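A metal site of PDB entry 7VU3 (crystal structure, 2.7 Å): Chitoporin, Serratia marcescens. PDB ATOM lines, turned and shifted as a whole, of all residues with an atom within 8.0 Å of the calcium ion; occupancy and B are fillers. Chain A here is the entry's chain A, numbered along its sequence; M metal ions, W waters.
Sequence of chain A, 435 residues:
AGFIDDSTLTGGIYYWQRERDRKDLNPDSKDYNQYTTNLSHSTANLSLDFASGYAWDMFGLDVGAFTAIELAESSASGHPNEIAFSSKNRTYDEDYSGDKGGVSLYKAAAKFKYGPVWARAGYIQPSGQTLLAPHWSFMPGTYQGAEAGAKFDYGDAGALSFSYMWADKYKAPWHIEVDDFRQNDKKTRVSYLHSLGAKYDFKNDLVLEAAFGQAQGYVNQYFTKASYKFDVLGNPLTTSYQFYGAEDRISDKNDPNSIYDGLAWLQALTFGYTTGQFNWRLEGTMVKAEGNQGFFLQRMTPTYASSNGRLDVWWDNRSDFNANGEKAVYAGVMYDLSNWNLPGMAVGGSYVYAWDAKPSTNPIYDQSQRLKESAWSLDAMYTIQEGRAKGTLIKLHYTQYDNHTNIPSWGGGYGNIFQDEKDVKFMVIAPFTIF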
ATOM      1  N   LYS A  23      -7.971  22.038 -26.837  1.00  0.00           N
ATOM      2  CA  LYS A  23      -6.863  22.919 -26.480  1.00  0.00           C
ATOM      3  C   LYS A  23      -5.801  22.928 -27.573  1.00  0.00           C
ATOM      4  O   LYS A  23      -5.470  21.880 -28.150  1.00  0.00           O
ATOM      5  CB  LYS A  23      -6.225  22.477 -25.164  1.00  0.00           C
ATOM      6  CG  LYS A  23      -6.711  23.217 -23.938  1.00  0.00           C
ATOM      7  CD  LYS A  23      -5.893  22.816 -22.719  1.00  0.00           C
ATOM      8  CE  LYS A  23      -6.603  23.146 -21.414  1.00  0.00           C
ATOM      9  NZ  LYS A  23      -6.031  22.395 -20.262  1.00  0.00           N
ATOM     10  N   LEU A  25      -1.962  23.463 -28.104  1.00  0.00           N
ATOM     11  CA  LEU A  25      -0.709  23.463 -27.360  1.00  0.00           C
ATOM     12  C   LEU A  25       0.492  23.813 -28.225  1.00  0.00           C
ATOM     13  O   LEU A  25       1.634  23.675 -27.769  1.00  0.00           O
ATOM     14  CB  LEU A  25      -0.496  22.101 -26.685  1.00  0.00           C
ATOM     15  CG  LEU A  25      -0.926  22.000 -25.220  1.00  0.00           C
ATOM     16  CD1 LEU A  25       0.044  22.765 -24.321  1.00  0.00           C
ATOM     17  CD2 LEU A  25      -2.349  22.503 -25.006  1.00  0.00           C
ATOM     18  N   ASN A  33      -2.857  27.381 -25.087  1.00  0.00           N
ATOM     19  CA  ASN A  33      -3.395  26.860 -23.830  1.00  0.00           C
ATOM     20  C   ASN A  33      -4.872  27.183 -23.629  1.00  0.00           C
ATOM     21  O   ASN A  33      -5.381  27.036 -22.518  1.00  0.00           O
ATOM     22  CB  ASN A  33      -2.585  27.374 -22.625  1.00  0.00           C
ATOM     23  CG  ASN A  33      -1.677  26.297 -22.046  1.00  0.00           C
ATOM     24  OD1 ASN A  33      -2.073  25.141 -21.906  1.00  0.00           O
ATOM     25  ND2 ASN A  33      -0.459  26.688 -21.699  1.00  0.00           N
ATOM     26  N   TYR A  35      -9.016  26.618 -25.033  1.00  0.00           N
ATOM     27  CA  TYR A  35      -9.891  25.767 -25.819  1.00  0.00           C
ATOM     28  C   TYR A  35     -10.339  26.502 -27.080  1.00  0.00           C
ATOM     29  O   TYR A  35     -10.729  27.671 -27.021  1.00  0.00           O
ATOM     30  CB  TYR A  35     -11.104  25.333 -25.005  1.00  0.00           C
ATOM     31  CG  TYR A  35     -10.785  24.323 -23.925  1.00  0.00           C
ATOM     32  CD1 TYR A  35     -10.806  22.953 -24.205  1.00  0.00           C
ATOM     33  CD2 TYR A  35     -10.470  24.723 -22.636  1.00  0.00           C
ATOM     34  CE1 TYR A  35     -10.516  22.026 -23.223  1.00  0.00           C
ATOM     35  CE2 TYR A  35     -10.186  23.806 -21.648  1.00  0.00           C
ATOM     36  CZ  TYR A  35     -10.206  22.459 -21.948  1.00  0.00           C
ATOM     37  OH  TYR A  35      -9.917  21.531 -20.967  1.00  0.00           O
ATOM     38  N   LYS A 372       0.064   9.894 -19.830  1.00  0.00           N
ATOM     39  CA  LYS A 372      -1.126   9.494 -19.111  1.00  0.00           C
ATOM     40  C   LYS A 372      -2.296  10.331 -19.582  1.00  0.00           C
ATOM     41  O   LYS A 372      -2.145  11.542 -19.801  1.00  0.00           O
ATOM     42  CB  LYS A 372      -0.942   9.645 -17.596  1.00  0.00           C
ATOM     43  CG  LYS A 372       0.078   8.676 -17.004  1.00  0.00           C
ATOM     44  CD  LYS A 372       0.598   9.147 -15.652  1.00  0.00           C
ATOM     45  CE  LYS A 372      -0.527   9.305 -14.646  1.00  0.00           C
ATOM     46  NZ  LYS A 372      -0.116   8.845 -13.292  1.00  0.00           N
ATOM     47  N   TYR A 401     -12.146  15.413 -21.515  1.00  0.00           N
ATOM     48  CA  TYR A 401     -10.968  14.581 -21.729  1.00  0.00           C
ATOM     49  C   TYR A 401      -9.711  15.375 -21.376  1.00  0.00           C
ATOM     50  O   TYR A 401      -9.569  16.532 -21.790  1.00  0.00           O
ATOM     51  CB  TYR A 401     -10.906  14.105 -23.178  1.00  0.00           C
ATOM     52  CG  TYR A 401      -9.546  13.582 -23.584  1.00  0.00           C
ATOM     53  CD1 TYR A 401      -9.135  12.305 -23.236  1.00  0.00           C
ATOM     54  CD2 TYR A 401      -8.678  14.373 -24.332  1.00  0.00           C
ATOM     55  CE1 TYR A 401      -7.894  11.835 -23.606  1.00  0.00           C
ATOM     56  CE2 TYR A 401      -7.437  13.903 -24.701  1.00  0.00           C
ATOM     57  CZ  TYR A 401      -7.053  12.633 -24.342  1.00  0.00           C
ATOM     58  OH  TYR A 401      -5.814  12.159 -24.720  1.00  0.00           O
ATOM     59  N   ASP A 402      -8.804  14.740 -20.639  1.00  0.00           N
ATOM     60  CA  ASP A 402      -7.584  15.400 -20.157  1.00  0.00           C
ATOM     61  C   ASP A 402      -6.361  14.658 -20.669  1.00  0.00           C
ATOM     62  O   ASP A 402      -6.191  13.470 -20.393  1.00  0.00           O
ATOM     63  CB  ASP A 402      -7.556  15.464 -18.628  1.00  0.00           C
ATOM     64  CG  ASP A 402      -6.426  16.320 -18.098  1.00  0.00           C
ATOM     65  OD1 ASP A 402      -5.740  16.992 -18.912  1.00  0.00           O
ATOM     66  OD2 ASP A 402      -6.217  16.349 -16.874  1.00  0.00           O
ATOM     67  N   ASN A 403      -5.529  15.372 -21.422  1.00  0.00           N
ATOM     68  CA  ASN A 403      -4.198  14.905 -21.826  1.00  0.00           C
ATOM     69  C   ASN A 403      -3.188  15.504 -20.861  1.00  0.00           C
ATOM     70  O   ASN A 403      -3.043  16.732 -20.779  1.00  0.00           O
ATOM     71  CB  ASN A 403      -3.909  15.319 -23.267  1.00  0.00           C
ATOM     72  CG  ASN A 403      -2.557  14.861 -23.754  1.00  0.00           C
ATOM     73  OD1 ASN A 403      -1.607  14.711 -22.982  1.00  0.00           O
ATOM     74  ND2 ASN A 403      -2.452  14.624 -25.061  1.00  0.00           N
ATOM     75  N   HIS A 404      -2.480  14.641 -20.118  1.00  0.00           N
ATOM     76  CA  HIS A 404      -1.590  15.087 -19.059  1.00  0.00           C
ATOM     77  C   HIS A 404      -0.185  15.418 -19.557  1.00  0.00           C
ATOM     78  O   HIS A 404       0.794  15.292 -18.799  1.00  0.00           O
ATOM     79  CB  HIS A 404      -1.516  14.023 -17.956  1.00  0.00           C
ATOM     80  CG  HIS A 404      -2.823  13.785 -17.269  1.00  0.00           C
ATOM     81  ND1 HIS A 404      -3.220  12.539 -16.826  1.00  0.00           N
ATOM     82  CD2 HIS A 404      -3.840  14.631 -16.951  1.00  0.00           C
ATOM     83  CE1 HIS A 404      -4.409  12.623 -16.274  1.00  0.00           C
ATOM     84  NE2 HIS A 404      -4.809  13.885 -16.341  1.00  0.00           N
ATOM     85  N   THR A 405      -0.048  15.847 -20.808  1.00  0.00           N
ATOM     86  CA  THR A 405       1.208  16.367 -21.336  1.00  0.00           C
ATOM     87  C   THR A 405       0.936  17.731 -21.960  1.00  0.00           C
ATOM     88  O   THR A 405      -0.183  18.246 -21.946  1.00  0.00           O
ATOM     89  CB  THR A 405       1.820  15.422 -22.380  1.00  0.00           C
ATOM     90  OG1 THR A 405       1.056  15.484 -23.590  1.00  0.00           O
ATOM     91  CG2 THR A 405       1.838  13.985 -21.865  1.00  0.00           C
ATOM     92  N   ASN A 406       1.998  18.330 -22.507  1.00  0.00           N
ATOM     93  CA  ASN A 406       1.891  19.520 -23.331  1.00  0.00           C
ATOM     94  C   ASN A 406       2.211  19.225 -24.795  1.00  0.00           C
ATOM     95  O   ASN A 406       2.413  20.169 -25.575  1.00  0.00           O
ATOM     96  CB  ASN A 406       2.802  20.624 -22.792  1.00  0.00           C
ATOM     97  CG  ASN A 406       2.431  21.049 -21.388  1.00  0.00           C
ATOM     98  OD1 ASN A 406       1.261  20.961 -20.994  1.00  0.00           O
ATOM     99  ND2 ASN A 406       3.415  21.490 -20.625  1.00  0.00           N
ATOM    100  N   PHE A 418      -4.797  13.330 -28.996  1.00  0.00           N
ATOM    101  CA  PHE A 418      -5.038  14.750 -29.121  1.00  0.00           C
ATOM    102  C   PHE A 418      -5.041  15.387 -27.739  1.00  0.00           C
ATOM    103  O   PHE A 418      -4.974  14.700 -26.711  1.00  0.00           O
ATOM    104  CB  PHE A 418      -6.356  15.033 -29.847  1.00  0.00           C
ATOM    105  CG  PHE A 418      -7.449  14.062 -29.496  1.00  0.00           C
ATOM    106  CD1 PHE A 418      -8.274  14.301 -28.412  1.00  0.00           C
ATOM    107  CD2 PHE A 418      -7.649  12.926 -30.249  1.00  0.00           C
ATOM    108  CE1 PHE A 418      -9.284  13.401 -28.081  1.00  0.00           C
ATOM    109  CE2 PHE A 418      -8.667  12.030 -29.930  1.00  0.00           C
ATOM    110  CZ  PHE A 418      -9.470  12.273 -28.850  1.00  0.00           C
ATOM    111  N   GLN A 419      -5.126  16.710 -27.700  1.00  0.00           N
ATOM    112  CA  GLN A 419      -5.038  17.458 -26.455  1.00  0.00           C
ATOM    113  C   GLN A 419      -6.401  17.544 -25.781  1.00  0.00           C
ATOM    114  O   GLN A 419      -7.402  17.019 -26.263  1.00  0.00           O
ATOM    115  CB  GLN A 419      -4.440  18.835 -26.718  1.00  0.00           C
ATOM    116  CG  GLN A 419      -2.938  18.884 -26.568  1.00  0.00           C
ATOM    117  CD  GLN A 419      -2.498  18.585 -25.145  1.00  0.00           C
ATOM    118  OE1 GLN A 419      -3.263  18.763 -24.207  1.00  0.00           O
ATOM    119  NE2 GLN A 419      -1.266  18.113 -24.996  1.00  0.00           N
ATOM    120  N   ASP A 420      -6.436  18.231 -24.636  1.00  0.00           N
ATOM    121  CA  ASP A 420      -7.630  18.284 -23.805  1.00  0.00           C
ATOM    122  C   ASP A 420      -8.842  18.672 -24.647  1.00  0.00           C
ATOM    123  O   ASP A 420      -8.733  19.464 -25.589  1.00  0.00           O
ATOM    124  CB  ASP A 420      -7.457  19.279 -22.658  1.00  0.00           C
ATOM    125  CG  ASP A 420      -6.272  18.915 -21.746  1.00  0.00           C
ATOM    126  OD1 ASP A 420      -5.815  17.758 -21.787  1.00  0.00           O
ATOM    127  OD2 ASP A 420      -5.816  19.793 -20.970  1.00  0.00           O
ATOM    128  N   GLU A 421     -10.002  18.117 -24.292  1.00  0.00           N
ATOM    129  CA  GLU A 421     -11.187  18.265 -25.131  1.00  0.00           C
ATOM    130  C   GLU A 421     -12.444  18.308 -24.277  1.00  0.00           C
ATOM    131  O   GLU A 421     -12.595  17.516 -23.339  1.00  0.00           O
ATOM    132  CB  GLU A 421     -11.276  17.113 -26.134  1.00  0.00           C
ATOM    133  CG  GLU A 421     -11.608  17.557 -27.547  1.00  0.00           C
ATOM    134  CD  GLU A 421     -11.503  16.418 -28.548  1.00  0.00           C
ATOM    135  OE1 GLU A 421     -12.124  15.350 -28.306  1.00  0.00           O
ATOM    136  OE2 GLU A 421     -10.805  16.585 -29.572  1.00  0.00           O
HETATM  137 CA    CA M   1      -4.108  18.620 -19.898  1.00  0.00          CA
HETATM  138  O   HOH W   1      -2.970  19.590 -21.749  1.00  0.00           O
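The calcium ion is bound by OD2 of Asp 420 (2.3 Å), O of Asn 403 (2.3 Å), water W1 (2.4 Å), OD1 of Asp 402 (2.5 Å) and OD1 of Asp 420 (2.7 Å). The calcium ion has five donor atoms within binding distance.
Water W1 lies within hydrogen-bond range of OE1 of Gln 419 (2.6 Å) and O of Thr 405 (3.1 Å).
A ring nitrogen (NE2) of His 404 lies within hydrogen-bond range of the side-chain carboxylate (OD2) of Asp 402. The side-chain amide nitrogen (ND2) of Asn 403 lies within hydrogen-bond range of the backbone carbonyl oxygen (O) of Phe 418. The backbone NH (N) of Lys 23 sits at hydrogen-bond distance from the backbone carbonyl oxygen (O) of Asp 420. The side-chain hydroxyl (OG1) of Thr 405 is in hydrogen-bond range of the side-chain amide oxygen (OD1) of Asn 403, 2.8 Å away.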
